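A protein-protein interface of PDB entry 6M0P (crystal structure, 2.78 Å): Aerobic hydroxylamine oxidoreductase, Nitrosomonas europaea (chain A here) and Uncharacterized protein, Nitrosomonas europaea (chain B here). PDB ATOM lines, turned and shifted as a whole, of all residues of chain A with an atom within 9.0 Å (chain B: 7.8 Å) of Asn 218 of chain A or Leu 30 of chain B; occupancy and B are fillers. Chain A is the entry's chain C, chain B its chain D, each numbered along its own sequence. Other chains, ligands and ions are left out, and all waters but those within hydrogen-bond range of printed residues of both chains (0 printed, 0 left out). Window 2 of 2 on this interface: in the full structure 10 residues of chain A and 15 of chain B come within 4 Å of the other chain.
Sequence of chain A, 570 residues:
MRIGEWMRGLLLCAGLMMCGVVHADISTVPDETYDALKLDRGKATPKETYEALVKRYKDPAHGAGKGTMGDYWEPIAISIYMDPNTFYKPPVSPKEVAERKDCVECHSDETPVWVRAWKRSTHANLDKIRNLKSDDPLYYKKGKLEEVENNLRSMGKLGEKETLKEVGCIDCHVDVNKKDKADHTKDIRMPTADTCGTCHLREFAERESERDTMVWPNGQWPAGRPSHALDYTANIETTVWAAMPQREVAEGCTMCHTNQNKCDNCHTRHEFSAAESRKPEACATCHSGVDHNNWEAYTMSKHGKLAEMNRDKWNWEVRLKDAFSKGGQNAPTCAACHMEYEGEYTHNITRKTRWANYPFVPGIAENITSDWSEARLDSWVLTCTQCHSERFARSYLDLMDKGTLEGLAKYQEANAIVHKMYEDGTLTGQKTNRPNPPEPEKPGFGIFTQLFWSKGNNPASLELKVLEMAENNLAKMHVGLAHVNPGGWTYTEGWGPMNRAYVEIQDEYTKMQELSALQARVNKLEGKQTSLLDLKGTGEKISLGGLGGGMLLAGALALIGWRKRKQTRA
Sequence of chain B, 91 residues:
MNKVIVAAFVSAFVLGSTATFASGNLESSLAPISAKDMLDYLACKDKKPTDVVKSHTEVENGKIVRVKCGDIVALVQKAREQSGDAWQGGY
The guanidinium group (NH2) of Arg 80 of chain B is in hydrogen-bond range of the backbone carbonyl oxygen (O) of Glu 366 of chain A. The backbone carbonyl oxygen (O) of Ser 28 of chain B is in hydrogen-bond range of the side-chain amide nitrogen (ND2) of Asn 218 of chain A (3.2 Å). The side-chain carboxylate (OE2) of Glu 366 of chain A lies within hydrogen-bond range of the backbone NH (N) of Ile 33 of chain B, 3.2 Å away. OG1 of Thr 369 of chain A is in hydrogen-bond range of NH2 of Arg 80 of chain B (3.2 Å).
OD1 of Asn 218 of chain A lies within hydrogen-bond range of ND2 of Asn 367 of chain A (3.3 Å). OG of Ser 83 of chain B is in hydrogen-bond range of N of Ala 31 of chain B. The backbone NH (N) of Asn 218 of chain A sits at hydrogen-bond distance from the side-chain amide oxygen (OE1) of Gln 220 of chain A (3.4 Å). The backbone carbonyl oxygen (O) of Ser 83 of chain B is in hydrogen-bond range of the side-chain hydroxyl (OG) of Ser 28 of chain B, at 3.2 Å. The side-chain carboxylate (OE1) of Glu 366 of chain A lies close to the backbone NH (N) of Gly 363 of chain A, at 3.2 Å.
Ser 29 of chain B touches Asn 218 of chain A. Asn 218 of chain A touches Leu 30 of chain B (OD1 to CD2, 3.7 Å). Ala 365 of chain A touches Met 38 of chain B (O to CE, 3.3 Å). CD2 of Leu 30 of chain B touches CB of Glu 366 of chain A, 3.7 Å away. Ala 31 of chain B touches Glu 366 of chain A. Pro 32 of chain B touches Glu 366 of chain A. CE of Met 38 of chain B touches CG2 of Thr 369 of chain A, 3.8 Å away.
Printed residues of chain B within 4 Å of Asn 218 of chain A: Ser 28 (3.2 Å), Ser 29 (3.98 Å) and Leu 30 (3.7 Å). Of chain A, only Asn 218 (3.7 Å) and Glu 366 (3.7 Å) come within 4 Å of Leu 30 of chain B. Of the printed residues of chain A, Ala 31 of chain B touches Glu 366. Printed residues of chain A within 4 Å of Ile 33 of chain B: Glu 366 (3.2 Å). Printed residues of chain A within 4 Å of Met 38 of chain B: Ala 365 and Thr 369. The nearest printed residue of chain B that does not touch Asn 218 of chain A is Ser 83 of chain B (6.4 Å). The nearest residue of chain A that does not touch Leu 30 of chain B is Asn 367 of chain A (4.3 Å).
Among the printed residues, 11 pairs touch across the chains.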
ATOM      1  N   VAL A 215     -16.332  10.807   9.906  1.00  0.00           N
ATOM      2  CA  VAL A 215     -16.114  10.189  11.206  1.00  0.00           C
ATOM      3  C   VAL A 215     -17.206  10.686  12.139  1.00  0.00           C
ATOM      4  O   VAL A 215     -17.286  11.888  12.423  1.00  0.00           O
ATOM      5  CB  VAL A 215     -14.722  10.505  11.778  1.00  0.00           C
ATOM      6  CG1 VAL A 215     -14.563   9.869  13.150  1.00  0.00           C
ATOM      7  CG2 VAL A 215     -13.639  10.015  10.831  1.00  0.00           C
ATOM      8  N   TRP A 216     -18.039   9.775  12.608  1.00  0.00           N
ATOM      9  CA  TRP A 216     -19.160  10.160  13.451  1.00  0.00           C
ATOM     10  C   TRP A 216     -18.694  10.360  14.892  1.00  0.00           C
ATOM     11  O   TRP A 216     -17.866   9.592  15.391  1.00  0.00           O
ATOM     12  CB  TRP A 216     -20.253   9.097  13.391  1.00  0.00           C
ATOM     13  CG  TRP A 216     -20.844   8.967  12.023  1.00  0.00           C
ATOM     14  CD1 TRP A 216     -20.380   8.192  11.000  1.00  0.00           C
ATOM     15  CD2 TRP A 216     -22.003   9.643  11.520  1.00  0.00           C
ATOM     16  NE1 TRP A 216     -21.180   8.340   9.893  1.00  0.00           N
ATOM     17  CE2 TRP A 216     -22.185   9.224  10.187  1.00  0.00           C
ATOM     18  CE3 TRP A 216     -22.905  10.558  12.068  1.00  0.00           C
ATOM     19  CZ2 TRP A 216     -23.230   9.691   9.394  1.00  0.00           C
ATOM     20  CZ3 TRP A 216     -23.944  11.018  11.279  1.00  0.00           C
ATOM     21  CH2 TRP A 216     -24.098  10.583   9.958  1.00  0.00           C
ATOM     22  N   PRO A 217     -19.206  11.387  15.579  1.00  0.00           N
ATOM     23  CA  PRO A 217     -18.705  11.682  16.931  1.00  0.00           C
ATOM     24  C   PRO A 217     -19.022  10.598  17.944  1.00  0.00           C
ATOM     25  O   PRO A 217     -18.216  10.363  18.852  1.00  0.00           O
ATOM     26  CB  PRO A 217     -19.401  13.004  17.280  1.00  0.00           C
ATOM     27  CG  PRO A 217     -20.637  13.008  16.443  1.00  0.00           C
ATOM     28  CD  PRO A 217     -20.260  12.327  15.159  1.00  0.00           C
ATOM     29  N   ASN A 218     -20.170   9.933  17.822  1.00  0.00           N
ATOM     30  CA  ASN A 218     -20.572   8.892  18.757  1.00  0.00           C
ATOM     31  C   ASN A 218     -20.567   7.506  18.124  1.00  0.00           C
ATOM     32  O   ASN A 218     -21.134   6.570  18.700  1.00  0.00           O
ATOM     33  CB  ASN A 218     -21.953   9.205  19.333  1.00  0.00           C
ATOM     34  CG  ASN A 218     -22.018  10.578  19.963  1.00  0.00           C
ATOM     35  OD1 ASN A 218     -22.732  11.460  19.486  1.00  0.00           O
ATOM     36  ND2 ASN A 218     -21.264  10.770  21.040  1.00  0.00           N
ATOM     37  N   GLY A 219     -19.946   7.353  16.960  1.00  0.00           N
ATOM     38  CA  GLY A 219     -19.880   6.060  16.302  1.00  0.00           C
ATOM     39  C   GLY A 219     -21.206   5.539  15.789  1.00  0.00           C
ATOM     40  O   GLY A 219     -21.473   4.334  15.892  1.00  0.00           O
ATOM     41  N   GLN A 220     -22.052   6.419  15.246  1.00  0.00           N
ATOM     42  CA  GLN A 220     -23.323   5.969  14.687  1.00  0.00           C
ATOM     43  C   GLN A 220     -23.106   5.038  13.501  1.00  0.00           C
ATOM     44  O   GLN A 220     -23.814   4.036  13.349  1.00  0.00           O
ATOM     45  CB  GLN A 220     -24.173   7.172  14.273  1.00  0.00           C
ATOM     46  CG  GLN A 220     -24.710   7.999  15.433  1.00  0.00           C
ATOM     47  CD  GLN A 220     -23.717   9.023  15.946  1.00  0.00           C
ATOM     48  OE1 GLN A 220     -22.542   9.003  15.584  1.00  0.00           O
ATOM     49  NE2 GLN A 220     -24.189   9.929  16.794  1.00  0.00           N
ATOM     50  N   TRP A 221     -22.139   5.357  12.648  1.00  0.00           N
ATOM     51  CA  TRP A 221     -21.724   4.524  11.534  1.00  0.00           C
ATOM     52  C   TRP A 221     -20.234   4.230  11.639  1.00  0.00           C
ATOM     53  O   TRP A 221     -19.499   4.948  12.329  1.00  0.00           O
ATOM     54  CB  TRP A 221     -22.018   5.203  10.188  1.00  0.00           C
ATOM     55  CG  TRP A 221     -23.462   5.509   9.948  1.00  0.00           C
ATOM     56  CD1 TRP A 221     -24.127   6.648  10.293  1.00  0.00           C
ATOM     57  CD2 TRP A 221     -24.422   4.665   9.302  1.00  0.00           C
ATOM     58  NE1 TRP A 221     -25.441   6.567   9.902  1.00  0.00           N
ATOM     59  CE2 TRP A 221     -25.648   5.357   9.293  1.00  0.00           C
ATOM     60  CE3 TRP A 221     -24.364   3.389   8.734  1.00  0.00           C
ATOM     61  CZ2 TRP A 221     -26.803   4.821   8.733  1.00  0.00           C
ATOM     62  CZ3 TRP A 221     -25.515   2.855   8.187  1.00  0.00           C
ATOM     63  CH2 TRP A 221     -26.716   3.570   8.187  1.00  0.00           C
ATOM     64  N   PRO A 222     -19.753   3.174  10.980  1.00  0.00           N
ATOM     65  CA  PRO A 222     -18.306   2.941  10.929  1.00  0.00           C
ATOM     66  C   PRO A 222     -17.582   4.124  10.301  1.00  0.00           C
ATOM     67  O   PRO A 222     -18.130   4.842   9.462  1.00  0.00           O
ATOM     68  CB  PRO A 222     -18.178   1.682  10.065  1.00  0.00           C
ATOM     69  CG  PRO A 222     -19.481   0.979  10.242  1.00  0.00           C
ATOM     70  CD  PRO A 222     -20.512   2.063  10.379  1.00  0.00           C
ATOM     71  N   VAL A 361     -31.185   4.870  12.968  1.00  0.00           N
ATOM     72  CA  VAL A 361     -29.884   4.398  13.453  1.00  0.00           C
ATOM     73  C   VAL A 361     -29.608   5.018  14.819  1.00  0.00           C
ATOM     74  O   VAL A 361     -29.765   6.243  14.982  1.00  0.00           O
ATOM     75  CB  VAL A 361     -28.786   4.746  12.451  1.00  0.00           C
ATOM     76  CG1 VAL A 361     -27.413   4.499  13.053  1.00  0.00           C
ATOM     77  CG2 VAL A 361     -28.969   3.934  11.183  1.00  0.00           C
ATOM     78  N   PRO A 362     -29.217   4.230  15.819  1.00  0.00           N
ATOM     79  CA  PRO A 362     -29.021   4.785  17.166  1.00  0.00           C
ATOM     80  C   PRO A 362     -27.964   5.878  17.171  1.00  0.00           C
ATOM     81  O   PRO A 362     -26.869   5.713  16.630  1.00  0.00           O
ATOM     82  CB  PRO A 362     -28.582   3.568  17.988  1.00  0.00           C
ATOM     83  CG  PRO A 362     -29.108   2.390  17.233  1.00  0.00           C
ATOM     84  CD  PRO A 362     -29.022   2.772  15.786  1.00  0.00           C
ATOM     85  N   GLY A 363     -28.308   7.006  17.788  1.00  0.00           N
ATOM     86  CA  GLY A 363     -27.414   8.135  17.881  1.00  0.00           C
ATOM     87  C   GLY A 363     -27.569   9.169  16.789  1.00  0.00           C
ATOM     88  O   GLY A 363     -27.047  10.280  16.935  1.00  0.00           O
ATOM     89  N   ILE A 364     -28.264   8.844  15.696  1.00  0.00           N
ATOM     90  CA  ILE A 364     -28.407   9.798  14.600  1.00  0.00           C
ATOM     91  C   ILE A 364     -29.323  10.944  15.007  1.00  0.00           C
ATOM     92  O   ILE A 364     -28.988  12.121  14.825  1.00  0.00           O
ATOM     93  CB  ILE A 364     -28.920   9.087  13.334  1.00  0.00           C
ATOM     94  CG1 ILE A 364     -27.828   8.193  12.747  1.00  0.00           C
ATOM     95  CG2 ILE A 364     -29.383  10.102  12.303  1.00  0.00           C
ATOM     96  CD1 ILE A 364     -26.619   8.953  12.253  1.00  0.00           C
ATOM     97  N   ALA A 365     -30.492  10.620  15.563  1.00  0.00           N
ATOM     98  CA  ALA A 365     -31.438  11.656  15.962  1.00  0.00           C
ATOM     99  C   ALA A 365     -30.904  12.479  17.127  1.00  0.00           C
ATOM    100  O   ALA A 365     -31.022  13.710  17.133  1.00  0.00           O
ATOM    101  CB  ALA A 365     -32.781  11.027  16.328  1.00  0.00           C
ATOM    102  N   GLU A 366     -30.311  11.816  18.121  1.00  0.00           N
ATOM    103  CA  GLU A 366     -29.789  12.516  19.287  1.00  0.00           C
ATOM    104  C   GLU A 366     -28.614  13.424  18.944  1.00  0.00           C
ATOM    105  O   GLU A 366     -28.324  14.355  19.703  1.00  0.00           O
ATOM    106  CB  GLU A 366     -29.376  11.504  20.357  1.00  0.00           C
ATOM    107  CG  GLU A 366     -30.494  10.559  20.798  1.00  0.00           C
ATOM    108  CD  GLU A 366     -30.646   9.344  19.896  1.00  0.00           C
ATOM    109  OE1 GLU A 366     -30.241   9.415  18.716  1.00  0.00           O
ATOM    110  OE2 GLU A 366     -31.172   8.314  20.369  1.00  0.00           O
ATOM    111  N   ASN A 367     -27.938  13.179  17.822  1.00  0.00           N
ATOM    112  CA  ASN A 367     -26.793  13.976  17.405  1.00  0.00           C
ATOM    113  C   ASN A 367     -27.182  15.167  16.536  1.00  0.00           C
ATOM    114  O   ASN A 367     -26.323  16.005  16.241  1.00  0.00           O
ATOM    115  CB  ASN A 367     -25.791  13.089  16.653  1.00  0.00           C
ATOM    116  CG  ASN A 367     -24.470  13.782  16.391  1.00  0.00           C
ATOM    117  OD1 ASN A 367     -24.177  14.175  15.263  1.00  0.00           O
ATOM    118  ND2 ASN A 367     -23.666  13.936  17.436  1.00  0.00           N
ATOM    119  N   ILE A 368     -28.451  15.273  16.135  1.00  0.00           N
ATOM    120  CA  ILE A 368     -28.852  16.321  15.205  1.00  0.00           C
ATOM    121  C   ILE A 368     -28.766  17.711  15.824  1.00  0.00           C
ATOM    122  O   ILE A 368     -28.723  18.706  15.092  1.00  0.00           O
ATOM    123  CB  ILE A 368     -30.269  16.043  14.669  1.00  0.00           C
ATOM    124  CG1 ILE A 368     -30.431  16.648  13.275  1.00  0.00           C
ATOM    125  CG2 ILE A 368     -31.323  16.596  15.616  1.00  0.00           C
ATOM    126  CD1 ILE A 368     -29.469  16.079  12.257  1.00  0.00           C
ATOM    127  N   THR A 369     -28.734  17.815  17.153  1.00  0.00           N
ATOM    128  CA  THR A 369     -28.608  19.104  17.822  1.00  0.00           C
ATOM    129  C   THR A 369     -27.186  19.392  18.284  1.00  0.00           C
ATOM    130  O   THR A 369     -26.946  20.442  18.888  1.00  0.00           O
ATOM    131  CB  THR A 369     -29.561  19.184  19.022  1.00  0.00           C
ATOM    132  OG1 THR A 369     -29.193  18.206  20.002  1.00  0.00           O
ATOM    133  CG2 THR A 369     -30.992  18.937  18.581  1.00  0.00           C
ATOM    134  N   SER A 370     -26.243  18.493  18.019  1.00  0.00           N
ATOM    135  CA  SER A 370     -24.873  18.707  18.449  1.00  0.00           C
ATOM    136  C   SER A 370     -24.193  19.755  17.573  1.00  0.00           C
ATOM    137  O   SER A 370     -24.648  20.078  16.472  1.00  0.00           O
ATOM    138  CB  SER A 370     -24.084  17.400  18.404  1.00  0.00           C
ATOM    139  OG  SER A 370     -23.953  16.936  17.072  1.00  0.00           O
ATOM    140  N   ASP A 371     -23.080  20.290  18.085  1.00  0.00           N
ATOM    141  CA  ASP A 371     -22.293  21.246  17.313  1.00  0.00           C
ATOM    142  C   ASP A 371     -21.691  20.603  16.071  1.00  0.00           C
ATOM    143  O   ASP A 371     -21.430  21.294  15.080  1.00  0.00           O
ATOM    144  CB  ASP A 371     -21.195  21.852  18.187  1.00  0.00           C
ATOM    145  CG  ASP A 371     -21.751  22.620  19.367  1.00  0.00           C
ATOM    146  OD1 ASP A 371     -22.801  23.278  19.205  1.00  0.00           O
ATOM    147  OD2 ASP A 371     -21.139  22.572  20.454  1.00  0.00           O
ATOM    148  N   TRP A 372     -21.456  19.290  16.109  1.00  0.00           N
ATOM    149  CA  TRP A 372     -20.966  18.586  14.928  1.00  0.00           C
ATOM    150  C   TRP A 372     -21.990  18.637  13.801  1.00  0.00           C
ATOM    151  O   TRP A 372     -21.648  18.912  12.645  1.00  0.00           O
ATOM    152  CB  TRP A 372     -20.628  17.140  15.291  1.00  0.00           C
ATOM    153  CG  TRP A 372     -20.060  16.337  14.161  1.00  0.00           C
ATOM    154  CD1 TRP A 372     -18.744  16.212  13.826  1.00  0.00           C
ATOM    155  CD2 TRP A 372     -20.791  15.539  13.223  1.00  0.00           C
ATOM    156  NE1 TRP A 372     -18.610  15.388  12.734  1.00  0.00           N
ATOM    157  CE2 TRP A 372     -19.853  14.962  12.345  1.00  0.00           C
ATOM    158  CE3 TRP A 372     -22.149  15.258  13.038  1.00  0.00           C
ATOM    159  CZ2 TRP A 372     -20.228  14.120  11.301  1.00  0.00           C
ATOM    160  CZ3 TRP A 372     -22.518  14.425  12.001  1.00  0.00           C
ATOM    161  CH2 TRP A 372     -21.562  13.865  11.145  1.00  0.00           C
ATOM    162  N   SER A 373     -23.260  18.377  14.123  1.00  0.00           N
ATOM    163  CA  SER A 373     -24.308  18.459  13.112  1.00  0.00           C
ATOM    164  C   SER A 373     -24.611  19.905  12.749  1.00  0.00           C
ATOM    165  O   SER A 373     -24.872  20.216  11.581  1.00  0.00           O
ATOM    166  CB  SER A 373     -25.572  17.756  13.607  1.00  0.00           C
ATOM    167  OG  SER A 373     -25.308  16.405  13.943  1.00  0.00           O
ATOM    168  N   SER B  28     -17.416   8.076  23.283  1.00  0.00           N
ATOM    169  CA  SER B  28     -18.327   7.016  23.697  1.00  0.00           C
ATOM    170  C   SER B  28     -19.676   7.143  22.994  1.00  0.00           C
ATOM    171  O   SER B  28     -19.927   8.113  22.278  1.00  0.00           O
ATOM    172  CB  SER B  28     -18.520   7.037  25.215  1.00  0.00           C
ATOM    173  OG  SER B  28     -19.080   8.267  25.643  1.00  0.00           O
ATOM    174  N   SER B  29     -20.540   6.153  23.204  1.00  0.00           N
ATOM    175  CA  SER B  29     -21.861   6.154  22.594  1.00  0.00           C
ATOM    176  C   SER B  29     -22.787   7.117  23.326  1.00  0.00           C
ATOM    177  O   SER B  29     -22.722   7.257  24.552  1.00  0.00           O
ATOM    178  CB  SER B  29     -22.454   4.745  22.602  1.00  0.00           C
ATOM    179  OG  SER B  29     -23.703   4.714  21.932  1.00  0.00           O
ATOM    180  N   LEU B  30     -23.651   7.783  22.566  1.00  0.00           N
ATOM    181  CA  LEU B  30     -24.557   8.774  23.126  1.00  0.00           C
ATOM    182  C   LEU B  30     -25.788   8.098  23.718  1.00  0.00           C
ATOM    183  O   LEU B  30     -26.234   7.048  23.249  1.00  0.00           O
ATOM    184  CB  LEU B  30     -24.973   9.782  22.053  1.00  0.00           C
ATOM    185  CG  LEU B  30     -25.687  11.049  22.525  1.00  0.00           C
ATOM    186  CD1 LEU B  30     -24.940  11.690  23.687  1.00  0.00           C
ATOM    187  CD2 LEU B  30     -25.837  12.032  21.376  1.00  0.00           C
ATOM    188  N   ALA B  31     -26.331   8.711  24.766  1.00  0.00           N
ATOM    189  CA  ALA B  31     -27.471   8.128  25.459  1.00  0.00           C
ATOM    190  C   ALA B  31     -28.724   8.220  24.591  1.00  0.00           C
ATOM    191  O   ALA B  31     -28.943   9.233  23.918  1.00  0.00           O
ATOM    192  CB  ALA B  31     -27.707   8.830  26.793  1.00  0.00           C
ATOM    193  N   PRO B  32     -29.560   7.184  24.584  1.00  0.00           N
ATOM    194  CA  PRO B  32     -30.744   7.195  23.719  1.00  0.00           C
ATOM    195  C   PRO B  32     -31.791   8.193  24.189  1.00  0.00           C
ATOM    196  O   PRO B  32     -32.052   8.338  25.385  1.00  0.00           O
ATOM    197  CB  PRO B  32     -31.271   5.757  23.813  1.00  0.00           C
ATOM    198  CG  PRO B  32     -30.129   4.952  24.369  1.00  0.00           C
ATOM    199  CD  PRO B  32     -29.385   5.890  25.263  1.00  0.00           C
ATOM    200  N   ILE B  33     -32.388   8.887  23.222  1.00  0.00           N
ATOM    201  CA  ILE B  33     -33.479   9.825  23.464  1.00  0.00           C
ATOM    202  C   ILE B  33     -34.535   9.587  22.395  1.00  0.00           C
ATOM    203  O   ILE B  33     -34.223   9.577  21.200  1.00  0.00           O
ATOM    204  CB  ILE B  33     -33.006  11.292  23.438  1.00  0.00           C
ATOM    205  CG1 ILE B  33     -31.974  11.547  24.539  1.00  0.00           C
ATOM    206  CG2 ILE B  33     -34.191  12.238  23.576  1.00  0.00           C
ATOM    207  CD1 ILE B  33     -31.404  12.950  24.529  1.00  0.00           C
ATOM    208  N   MET B  38     -36.996  14.498  21.466  1.00  0.00           N
ATOM    209  CA  MET B  38     -36.192  15.402  20.651  1.00  0.00           C
ATOM    210  C   MET B  38     -37.039  16.533  20.081  1.00  0.00           C
ATOM    211  O   MET B  38     -36.593  17.685  20.024  1.00  0.00           O
ATOM    212  CB  MET B  38     -35.501  14.629  19.531  1.00  0.00           C
ATOM    213  CG  MET B  38     -34.426  13.681  20.024  1.00  0.00           C
ATOM    214  SD  MET B  38     -33.040  14.568  20.757  1.00  0.00           S
ATOM    215  CE  MET B  38     -32.538  15.609  19.390  1.00  0.00           C
ATOM    216  N   ALA B  79     -30.102  12.777  30.429  1.00  0.00           N
ATOM    217  CA  ALA B  79     -29.555  11.735  29.572  1.00  0.00           C
ATOM    218  C   ALA B  79     -28.181  12.098  29.031  1.00  0.00           C
ATOM    219  O   ALA B  79     -27.354  11.207  28.809  1.00  0.00           O
ATOM    220  CB  ALA B  79     -30.509  11.450  28.409  1.00  0.00           C
ATOM    221  N   ARG B  80     -27.911  13.390  28.832  1.00  0.00           N
ATOM    222  CA  ARG B  80     -26.599  13.805  28.346  1.00  0.00           C
ATOM    223  C   ARG B  80     -25.520  13.594  29.399  1.00  0.00           C
ATOM    224  O   ARG B  80     -24.369  13.305  29.052  1.00  0.00           O
ATOM    225  CB  ARG B  80     -26.638  15.266  27.895  1.00  0.00           C
ATOM    226  CG  ARG B  80     -27.585  15.523  26.733  1.00  0.00           C
ATOM    227  CD  ARG B  80     -27.103  14.831  25.463  1.00  0.00           C
ATOM    228  NE  ARG B  80     -28.013  15.046  24.340  1.00  0.00           N
ATOM    229  CZ  ARG B  80     -27.941  16.074  23.501  1.00  0.00           C
ATOM    230  NH1 ARG B  80     -26.994  16.992  23.650  1.00  0.00           N
ATOM    231  NH2 ARG B  80     -28.816  16.185  22.511  1.00  0.00           N
ATOM    232  N   GLU B  81     -25.866  13.728  30.680  1.00  0.00           N
ATOM    233  CA  GLU B  81     -24.890  13.532  31.744  1.00  0.00           C
ATOM    234  C   GLU B  81     -24.540  12.064  31.946  1.00  0.00           C
ATOM    235  O   GLU B  81     -23.549  11.768  32.621  1.00  0.00           O
ATOM    236  CB  GLU B  81     -25.403  14.140  33.054  1.00  0.00           C
ATOM    237  CG  GLU B  81     -26.765  13.632  33.511  1.00  0.00           C
ATOM    238  CD  GLU B  81     -26.670  12.424  34.425  1.00  0.00           C
ATOM    239  OE1 GLU B  81     -25.546  12.083  34.849  1.00  0.00           O
ATOM    240  OE2 GLU B  81     -27.721  11.819  34.724  1.00  0.00           O
ATOM    241  N   GLN B  82     -25.325  11.146  31.381  1.00  0.00           N
ATOM    242  CA  GLN B  82     -25.036   9.721  31.427  1.00  0.00           C
ATOM    243  C   GLN B  82     -24.195   9.262  30.242  1.00  0.00           C
ATOM    244  O   GLN B  82     -24.113   8.056  29.980  1.00  0.00           O
ATOM    245  CB  GLN B  82     -26.340   8.921  31.481  1.00  0.00           C
ATOM    246  CG  GLN B  82     -27.161   9.144  32.737  1.00  0.00           C
ATOM    247  CD  GLN B  82     -28.466   8.372  32.720  1.00  0.00           C
ATOM    248  OE1 GLN B  82     -28.733   7.602  31.797  1.00  0.00           O
ATOM    249  NE2 GLN B  82     -29.288   8.575  33.742  1.00  0.00           N
ATOM    250  N   SER B  83     -23.572  10.192  29.524  1.00  0.00           N
ATOM    251  CA  SER B  83     -22.776   9.859  28.349  1.00  0.00           C
ATOM    252  C   SER B  83     -21.286  10.032  28.628  1.00  0.00           C
ATOM    253  O   SER B  83     -20.487  10.196  27.705  1.00  0.00           O
ATOM    254  CB  SER B  83     -23.190  10.724  27.157  1.00  0.00           C
ATOM    255  OG  SER B  83     -24.564  10.555  26.855  1.00  0.00           O
